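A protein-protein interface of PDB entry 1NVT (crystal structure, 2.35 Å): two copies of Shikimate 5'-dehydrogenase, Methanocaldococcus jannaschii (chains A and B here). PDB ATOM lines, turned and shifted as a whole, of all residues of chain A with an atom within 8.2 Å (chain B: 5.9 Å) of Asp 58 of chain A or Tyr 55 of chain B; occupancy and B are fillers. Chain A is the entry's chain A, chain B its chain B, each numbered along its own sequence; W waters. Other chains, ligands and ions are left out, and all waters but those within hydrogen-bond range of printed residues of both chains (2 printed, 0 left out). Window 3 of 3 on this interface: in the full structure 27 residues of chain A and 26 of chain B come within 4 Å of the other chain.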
ATOM      1  N   LEU A  53     -13.210  14.595 -26.627  1.00  0.00           N
ATOM      2  CA  LEU A  53     -12.515  14.943 -27.857  1.00  0.00           C
ATOM      3  C   LEU A  53     -12.036  16.393 -27.844  1.00  0.00           C
ATOM      4  O   LEU A  53     -11.004  16.728 -28.432  1.00  0.00           O
ATOM      5  CB  LEU A  53     -13.420  14.704 -29.068  1.00  0.00           C
ATOM      6  CG  LEU A  53     -12.667  14.784 -30.401  1.00  0.00           C
ATOM      7  CD1 LEU A  53     -11.582  13.715 -30.443  1.00  0.00           C
ATOM      8  CD2 LEU A  53     -13.634  14.614 -31.564  1.00  0.00           C
ATOM      9  N   LYS A  54     -12.774  17.248 -27.150  1.00  0.00           N
ATOM     10  CA  LYS A  54     -12.424  18.660 -27.075  1.00  0.00           C
ATOM     11  C   LYS A  54     -11.103  18.935 -26.349  1.00  0.00           C
ATOM     12  O   LYS A  54     -10.578  20.040 -26.430  1.00  0.00           O
ATOM     13  CB  LYS A  54     -13.557  19.447 -26.395  1.00  0.00           C
ATOM     14  CG  LYS A  54     -13.759  19.089 -24.928  1.00  0.00           C
ATOM     15  CD  LYS A  54     -14.778  20.005 -24.230  1.00  0.00           C
ATOM     16  CE  LYS A  54     -16.202  19.668 -24.630  1.00  0.00           C
ATOM     17  NZ  LYS A  54     -16.627  18.322 -24.130  1.00  0.00           N
ATOM     18  N   TYR A  55     -10.557  17.941 -25.653  1.00  0.00           N
ATOM     19  CA  TYR A  55      -9.306  18.139 -24.912  1.00  0.00           C
ATOM     20  C   TYR A  55      -8.051  17.556 -25.555  1.00  0.00           C
ATOM     21  O   TYR A  55      -6.944  17.783 -25.060  1.00  0.00           O
ATOM     22  CB  TYR A  55      -9.405  17.526 -23.519  1.00  0.00           C
ATOM     23  CG  TYR A  55     -10.563  18.000 -22.676  1.00  0.00           C
ATOM     24  CD1 TYR A  55     -11.500  17.092 -22.195  1.00  0.00           C
ATOM     25  CD2 TYR A  55     -10.701  19.348 -22.324  1.00  0.00           C
ATOM     26  CE1 TYR A  55     -12.547  17.500 -21.382  1.00  0.00           C
ATOM     27  CE2 TYR A  55     -11.753  19.774 -21.505  1.00  0.00           C
ATOM     28  CZ  TYR A  55     -12.669  18.837 -21.038  1.00  0.00           C
ATOM     29  OH  TYR A  55     -13.703  19.212 -20.211  1.00  0.00           O
ATOM     30  N   VAL A  56      -8.205  16.816 -26.647  1.00  0.00           N
ATOM     31  CA  VAL A  56      -7.049  16.169 -27.249  1.00  0.00           C
ATOM     32  C   VAL A  56      -6.038  17.046 -27.970  1.00  0.00           C
ATOM     33  O   VAL A  56      -4.836  16.910 -27.735  1.00  0.00           O
ATOM     34  CB  VAL A  56      -7.479  15.003 -28.194  1.00  0.00           C
ATOM     35  CG1 VAL A  56      -8.445  14.088 -27.463  1.00  0.00           C
ATOM     36  CG2 VAL A  56      -8.121  15.535 -29.454  1.00  0.00           C
ATOM     37  N   ILE A  57      -6.498  17.944 -28.831  1.00  0.00           N
ATOM     38  CA  ILE A  57      -5.571  18.783 -29.573  1.00  0.00           C
ATOM     39  C   ILE A  57      -4.669  19.601 -28.660  1.00  0.00           C
ATOM     40  O   ILE A  57      -3.448  19.557 -28.796  1.00  0.00           O
ATOM     41  CB  ILE A  57      -6.313  19.715 -30.541  1.00  0.00           C
ATOM     42  CG1 ILE A  57      -7.077  18.878 -31.574  1.00  0.00           C
ATOM     43  CG2 ILE A  57      -5.321  20.630 -31.246  1.00  0.00           C
ATOM     44  CD1 ILE A  57      -6.200  17.972 -32.422  1.00  0.00           C
ATOM     45  N   ASP A  58      -5.251  20.339 -27.723  1.00  0.00           N
ATOM     46  CA  ASP A  58      -4.424  21.129 -26.816  1.00  0.00           C
ATOM     47  C   ASP A  58      -3.566  20.248 -25.910  1.00  0.00           C
ATOM     48  O   ASP A  58      -2.551  20.692 -25.388  1.00  0.00           O
ATOM     49  CB  ASP A  58      -5.289  22.062 -25.965  1.00  0.00           C
ATOM     50  CG  ASP A  58      -5.915  23.174 -26.787  1.00  0.00           C
ATOM     51  OD1 ASP A  58      -5.234  23.684 -27.706  1.00  0.00           O
ATOM     52  OD2 ASP A  58      -7.078  23.542 -26.515  1.00  0.00           O
ATOM     53  N   GLY A  59      -3.971  18.998 -25.721  1.00  0.00           N
ATOM     54  CA  GLY A  59      -3.184  18.115 -24.880  1.00  0.00           C
ATOM     55  C   GLY A  59      -1.985  17.648 -25.681  1.00  0.00           C
ATOM     56  O   GLY A  59      -0.851  17.593 -25.187  1.00  0.00           O
ATOM     57  N   ALA A  60      -2.242  17.312 -26.940  1.00  0.00           N
ATOM     58  CA  ALA A  60      -1.189  16.856 -27.828  1.00  0.00           C
ATOM     59  C   ALA A  60      -0.149  17.964 -28.015  1.00  0.00           C
ATOM     60  O   ALA A  60       1.058  17.704 -28.021  1.00  0.00           O
ATOM     61  CB  ALA A  60      -1.781  16.468 -29.160  1.00  0.00           C
ATOM     62  N   LYS A  61      -0.625  19.199 -28.164  1.00  0.00           N
ATOM     63  CA  LYS A  61       0.265  20.339 -28.358  1.00  0.00           C
ATOM     64  C   LYS A  61       1.115  20.559 -27.129  1.00  0.00           C
ATOM     65  O   LYS A  61       2.319  20.793 -27.231  1.00  0.00           O
ATOM     66  CB  LYS A  61      -0.535  21.614 -28.655  1.00  0.00           C
ATOM     67  CG  LYS A  61      -1.115  21.667 -30.057  1.00  0.00           C
ATOM     68  CD  LYS A  61      -1.938  22.928 -30.263  1.00  0.00           C
ATOM     69  CE  LYS A  61      -2.402  23.049 -31.714  1.00  0.00           C
ATOM     70  NZ  LYS A  61      -3.354  24.187 -31.894  1.00  0.00           N
ATOM     71  N   ALA A  62       0.481  20.480 -25.968  1.00  0.00           N
ATOM     72  CA  ALA A  62       1.175  20.664 -24.708  1.00  0.00           C
ATOM     73  C   ALA A  62       2.200  19.552 -24.457  1.00  0.00           C
ATOM     74  O   ALA A  62       3.287  19.799 -23.928  1.00  0.00           O
ATOM     75  CB  ALA A  62       0.174  20.695 -23.594  1.00  0.00           C
ATOM     76  N   LEU A  63       1.849  18.332 -24.855  1.00  0.00           N
ATOM     77  CA  LEU A  63       2.701  17.170 -24.641  1.00  0.00           C
ATOM     78  C   LEU A  63       3.794  17.007 -25.670  1.00  0.00           C
ATOM     79  O   LEU A  63       4.853  16.471 -25.372  1.00  0.00           O
ATOM     80  CB  LEU A  63       1.846  15.894 -24.612  1.00  0.00           C
ATOM     81  CG  LEU A  63       0.936  15.761 -23.392  1.00  0.00           C
ATOM     82  CD1 LEU A  63      -0.027  14.594 -23.564  1.00  0.00           C
ATOM     83  CD2 LEU A  63       1.802  15.581 -22.165  1.00  0.00           C
ATOM     84  N   GLY A  64       3.547  17.461 -26.887  1.00  0.00           N
ATOM     85  CA  GLY A  64       4.565  17.315 -27.901  1.00  0.00           C
ATOM     86  C   GLY A  64       4.292  16.088 -28.739  1.00  0.00           C
ATOM     87  O   GLY A  64       5.194  15.553 -29.404  1.00  0.00           O
ATOM     88  N   PHE A  68      -1.643  12.209 -35.128  1.00  0.00           N
ATOM     89  CA  PHE A  68      -2.620  11.164 -34.871  1.00  0.00           C
ATOM     90  C   PHE A  68      -3.229  10.644 -36.149  1.00  0.00           C
ATOM     91  O   PHE A  68      -3.092  11.218 -37.234  1.00  0.00           O
ATOM     92  CB  PHE A  68      -3.845  11.670 -34.097  1.00  0.00           C
ATOM     93  CG  PHE A  68      -3.563  12.214 -32.740  1.00  0.00           C
ATOM     94  CD1 PHE A  68      -3.520  13.589 -32.528  1.00  0.00           C
ATOM     95  CD2 PHE A  68      -3.419  11.363 -31.651  1.00  0.00           C
ATOM     96  CE1 PHE A  68      -3.341  14.111 -31.241  1.00  0.00           C
ATOM     97  CE2 PHE A  68      -3.237  11.874 -30.361  1.00  0.00           C
ATOM     98  CZ  PHE A  68      -3.201  13.252 -30.156  1.00  0.00           C
ATOM     99  N   ILE A  78     -13.613  16.035 -34.982  1.00  0.00           N
ATOM    100  CA  ILE A  78     -12.270  16.528 -34.653  1.00  0.00           C
ATOM    101  C   ILE A  78     -11.958  17.806 -35.449  1.00  0.00           C
ATOM    102  O   ILE A  78     -11.181  18.648 -35.013  1.00  0.00           O
ATOM    103  CB  ILE A  78     -11.175  15.449 -34.976  1.00  0.00           C
ATOM    104  CG1 ILE A  78      -9.814  15.868 -34.427  1.00  0.00           C
ATOM    105  CG2 ILE A  78     -11.022  15.295 -36.478  1.00  0.00           C
ATOM    106  CD1 ILE A  78      -9.772  15.981 -32.943  1.00  0.00           C
ATOM    107  N   TYR A  81     -11.659  21.318 -33.952  1.00  0.00           N
ATOM    108  CA  TYR A  81     -10.609  21.530 -32.960  1.00  0.00           C
ATOM    109  C   TYR A  81      -9.239  21.747 -33.595  1.00  0.00           C
ATOM    110  O   TYR A  81      -8.264  22.038 -32.901  1.00  0.00           O
ATOM    111  CB  TYR A  81     -10.565  20.336 -32.003  1.00  0.00           C
ATOM    112  CG  TYR A  81     -11.860  20.152 -31.247  1.00  0.00           C
ATOM    113  CD1 TYR A  81     -12.263  21.077 -30.283  1.00  0.00           C
ATOM    114  CD2 TYR A  81     -12.704  19.073 -31.517  1.00  0.00           C
ATOM    115  CE1 TYR A  81     -13.477  20.936 -29.609  1.00  0.00           C
ATOM    116  CE2 TYR A  81     -13.924  18.923 -30.847  1.00  0.00           C
ATOM    117  CZ  TYR A  81     -14.301  19.859 -29.897  1.00  0.00           C
ATOM    118  OH  TYR A  81     -15.507  19.727 -29.242  1.00  0.00           O
ATOM    119  N   ASP A  83      -6.505  23.594 -36.412  1.00  0.00           N
ATOM    120  CA  ASP A  83      -6.170  24.941 -36.872  1.00  0.00           C
ATOM    121  C   ASP A  83      -6.369  25.104 -38.373  1.00  0.00           C
ATOM    122  O   ASP A  83      -6.727  26.181 -38.848  1.00  0.00           O
ATOM    123  CB  ASP A  83      -4.715  25.262 -36.533  1.00  0.00           C
ATOM    124  CG  ASP A  83      -4.477  25.385 -35.047  1.00  0.00           C
ATOM    125  OD1 ASP A  83      -4.870  26.421 -34.469  1.00  0.00           O
ATOM    126  OD2 ASP A  83      -3.900  24.443 -34.457  1.00  0.00           O
ATOM    127  N   ILE A 100       0.796  17.823 -35.970  1.00  0.00           N
ATOM    128  CA  ILE A 100       0.926  19.003 -35.127  1.00  0.00           C
ATOM    129  C   ILE A 100       2.349  19.543 -35.269  1.00  0.00           C
ATOM    130  O   ILE A 100       3.319  18.840 -34.981  1.00  0.00           O
ATOM    131  CB  ILE A 100       0.653  18.666 -33.647  1.00  0.00           C
ATOM    132  CG1 ILE A 100      -0.791  18.176 -33.491  1.00  0.00           C
ATOM    133  CG2 ILE A 100       0.912  19.895 -32.770  1.00  0.00           C
ATOM    134  CD1 ILE A 100      -1.178  17.840 -32.079  1.00  0.00           C
ATOM    135  N   GLY A 103       2.724  24.673 -33.083  1.00  0.00           N
ATOM    136  CA  GLY A 103       1.492  25.096 -32.438  1.00  0.00           C
ATOM    137  C   GLY A 103       0.264  24.996 -33.315  1.00  0.00           C
ATOM    138  O   GLY A 103      -0.838  25.322 -32.878  1.00  0.00           O
ATOM    139  N   ALA A 105      -2.230  22.568 -35.564  1.00  0.00           N
ATOM    140  CA  ALA A 105      -2.672  21.196 -35.795  1.00  0.00           C
ATOM    141  C   ALA A 105      -3.390  21.181 -37.140  1.00  0.00           C
ATOM    142  O   ALA A 105      -4.414  21.846 -37.310  1.00  0.00           O
ATOM    143  CB  ALA A 105      -3.617  20.743 -34.681  1.00  0.00           C
ATOM    144  N   GLU B  51       3.852  27.193 -19.752  1.00  0.00           N
ATOM    145  CA  GLU B  51       2.636  27.851 -20.221  1.00  0.00           C
ATOM    146  C   GLU B  51       1.565  26.877 -20.707  1.00  0.00           C
ATOM    147  O   GLU B  51       0.386  27.224 -20.782  1.00  0.00           O
ATOM    148  CB  GLU B  51       2.980  28.841 -21.342  1.00  0.00           C
ATOM    149  CG  GLU B  51       3.758  28.214 -22.486  1.00  0.00           C
ATOM    150  CD  GLU B  51       5.208  28.677 -22.550  1.00  0.00           C
ATOM    151  OE1 GLU B  51       5.855  28.801 -21.485  1.00  0.00           O
ATOM    152  OE2 GLU B  51       5.707  28.900 -23.677  1.00  0.00           O
ATOM    153  N   ASN B  52       1.971  25.656 -21.032  1.00  0.00           N
ATOM    154  CA  ASN B  52       1.029  24.656 -21.515  1.00  0.00           C
ATOM    155  C   ASN B  52       0.685  23.599 -20.482  1.00  0.00           C
ATOM    156  O   ASN B  52      -0.142  22.730 -20.738  1.00  0.00           O
ATOM    157  CB  ASN B  52       1.596  23.982 -22.758  1.00  0.00           C
ATOM    158  CG  ASN B  52       1.679  24.926 -23.925  1.00  0.00           C
ATOM    159  OD1 ASN B  52       2.342  24.643 -24.925  1.00  0.00           O
ATOM    160  ND2 ASN B  52       0.989  26.060 -23.814  1.00  0.00           N
ATOM    161  N   LEU B  53       1.310  23.676 -19.317  1.00  0.00           N
ATOM    162  CA  LEU B  53       1.065  22.697 -18.270  1.00  0.00           C
ATOM    163  C   LEU B  53      -0.417  22.500 -17.961  1.00  0.00           C
ATOM    164  O   LEU B  53      -0.836  21.405 -17.585  1.00  0.00           O
ATOM    165  CB  LEU B  53       1.795  23.101 -16.986  1.00  0.00           C
ATOM    166  CG  LEU B  53       1.718  22.100 -15.830  1.00  0.00           C
ATOM    167  CD1 LEU B  53       2.376  20.779 -16.223  1.00  0.00           C
ATOM    168  CD2 LEU B  53       2.405  22.683 -14.622  1.00  0.00           C
ATOM    169  N   LYS B  54      -1.202  23.559 -18.125  1.00  0.00           N
ATOM    170  CA  LYS B  54      -2.630  23.516 -17.823  1.00  0.00           C
ATOM    171  C   LYS B  54      -3.481  22.649 -18.748  1.00  0.00           C
ATOM    172  O   LYS B  54      -4.635  22.352 -18.427  1.00  0.00           O
ATOM    173  CB  LYS B  54      -3.202  24.939 -17.800  1.00  0.00           C
ATOM    174  CG  LYS B  54      -3.176  25.646 -19.144  1.00  0.00           C
ATOM    175  CD  LYS B  54      -3.767  27.046 -19.030  1.00  0.00           C
ATOM    176  CE  LYS B  54      -3.756  27.780 -20.368  1.00  0.00           C
ATOM    177  NZ  LYS B  54      -4.302  29.170 -20.238  1.00  0.00           N
ATOM    178  N   TYR B  55      -2.927  22.238 -19.887  1.00  0.00           N
ATOM    179  CA  TYR B  55      -3.676  21.410 -20.829  1.00  0.00           C
ATOM    180  C   TYR B  55      -3.387  19.913 -20.700  1.00  0.00           C
ATOM    181  O   TYR B  55      -4.094  19.102 -21.291  1.00  0.00           O
ATOM    182  CB  TYR B  55      -3.365  21.815 -22.274  1.00  0.00           C
ATOM    183  CG  TYR B  55      -3.634  23.257 -22.625  1.00  0.00           C
ATOM    184  CD1 TYR B  55      -4.911  23.809 -22.502  1.00  0.00           C
ATOM    185  CD2 TYR B  55      -2.612  24.065 -23.118  1.00  0.00           C
ATOM    186  CE1 TYR B  55      -5.159  25.139 -22.871  1.00  0.00           C
ATOM    187  CE2 TYR B  55      -2.844  25.387 -23.488  1.00  0.00           C
ATOM    188  CZ  TYR B  55      -4.114  25.919 -23.365  1.00  0.00           C
ATOM    189  OH  TYR B  55      -4.327  27.222 -23.753  1.00  0.00           O
ATOM    190  N   VAL B  56      -2.370  19.548 -19.924  1.00  0.00           N
ATOM    191  CA  VAL B  56      -1.957  18.144 -19.796  1.00  0.00           C
ATOM    192  C   VAL B  56      -2.873  17.127 -19.095  1.00  0.00           C
ATOM    193  O   VAL B  56      -3.057  16.018 -19.602  1.00  0.00           O
ATOM    194  CB  VAL B  56      -0.548  18.039 -19.139  1.00  0.00           C
ATOM    195  CG1 VAL B  56       0.448  18.922 -19.879  1.00  0.00           C
ATOM    196  CG2 VAL B  56      -0.620  18.447 -17.702  1.00  0.00           C
ATOM    197  N   ILE B  57      -3.431  17.481 -17.943  1.00  0.00           N
ATOM    198  CA  ILE B  57      -4.284  16.551 -17.216  1.00  0.00           C
ATOM    199  C   ILE B  57      -5.576  16.208 -17.957  1.00  0.00           C
ATOM    200  O   ILE B  57      -5.965  15.044 -18.029  1.00  0.00           O
ATOM    201  CB  ILE B  57      -4.611  17.092 -15.807  1.00  0.00           C
ATOM    202  CG1 ILE B  57      -3.325  17.158 -14.984  1.00  0.00           C
ATOM    203  CG2 ILE B  57      -5.607  16.194 -15.112  1.00  0.00           C
ATOM    204  CD1 ILE B  57      -2.589  15.813 -14.878  1.00  0.00           C
ATOM    205  N   ASP B  58      -6.251  17.211 -18.500  1.00  0.00           N
ATOM    206  CA  ASP B  58      -7.472  16.951 -19.251  1.00  0.00           C
ATOM    207  C   ASP B  58      -7.069  16.165 -20.498  1.00  0.00           C
ATOM    208  O   ASP B  58      -7.791  15.281 -20.946  1.00  0.00           O
ATOM    209  CB  ASP B  58      -8.154  18.265 -19.639  1.00  0.00           C
ATOM    210  CG  ASP B  58      -8.937  18.879 -18.487  1.00  0.00           C
ATOM    211  OD1 ASP B  58      -9.034  20.129 -18.421  1.00  0.00           O
ATOM    212  OD2 ASP B  58      -9.468  18.112 -17.654  1.00  0.00           O
ATOM    213  N   GLY B  59      -5.896  16.483 -21.042  1.00  0.00           N
ATOM    214  CA  GLY B  59      -5.425  15.785 -22.221  1.00  0.00           C
ATOM    215  C   GLY B  59      -5.203  14.329 -21.873  1.00  0.00           C
ATOM    216  O   GLY B  59      -5.660  13.430 -22.586  1.00  0.00           O
ATOM    217  N   ALA B  60      -4.506  14.099 -20.765  1.00  0.00           N
ATOM    218  CA  ALA B  60      -4.234  12.748 -20.310  1.00  0.00           C
ATOM    219  C   ALA B  60      -5.544  11.987 -20.097  1.00  0.00           C
ATOM    220  O   ALA B  60      -5.695  10.850 -20.561  1.00  0.00           O
ATOM    221  CB  ALA B  60      -3.432  12.787 -19.013  1.00  0.00           C
HETATM  222  O   HOH W   1       4.519  22.411 -24.062  1.00  0.00           O
HETATM  223  O   HOH W   2      -6.371  19.504 -22.977  1.00  0.00           O
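Among the printed residues, merely in contact across the chains: Asp 58 of chain A with Tyr 55 of chain B, Ala 62 of chain A with Asn 52 of chain B, Tyr 55 of chain A with Asp 58 of chain B, Tyr 55 of chain A with Gly 59 of chain B, Gly 59 of chain A with Tyr 55 of chain B and Ala 62 of chain A with Tyr 55 of chain B.
Tyr 55 of chain A touches Asp 58 of chain B, and with the chains exchanged Asp 58 of chain A touches Tyr 55 of chain B. Tyr 55 of chain A touches Gly 59 of chain B, and with the chains exchanged Gly 59 of chain A touches Tyr 55 of chain B. Positions printed for both chains: 53, 54, 55, 56, 57, 58, 59 and 60.
Lys 61 of chain A touches none of the printed residues of chain B. Printed residues of chain B within 4 Å of Ala 62 of chain A: Asn 52 and Tyr 55. Glu 51 of chain B touches none of the printed residues of chain A. Printed residues of chain A within 4 Å of Asn 52 of chain B: Ala 62. The nearest residue of chain B that does not touch Asp 58 of chain A is Val 56 of chain B (5.6 Å).
Printed residues of chain A that touch a printed residue of chain B: Tyr 55, Asp 58, Gly 59 and Ala 62. Hydrophobic or aromatic side chains of chain A that line the printed part of chain B: Tyr 55 and Ala 62. Printed residues of chain B that touch a printed residue of chain A: Asn 52, Tyr 55, Asp 58 and Gly 59. Hydrophobic or aromatic side chains of chain B that line the printed part of chain A: Tyr 55. Among the printed residues, 6 pairs touch across the chains. Among the printed residues, no Asp or Glu carboxylate lies within 4 Å of a Lys or Arg side-chain nitrogen of the other chain.
Water W2 bridges the backbone carbonyl oxygen (O) of Tyr 55 of chain A (2.8 Å) and the backbone carbonyl oxygen (O) of Tyr 55 of chain B (2.9 Å). Water W1 bridges the backbone carbonyl oxygen of Ala 62 of chain A (2.9 Å) and the side-chain amide oxygen of Asn 52 of chain B (3.2 Å).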
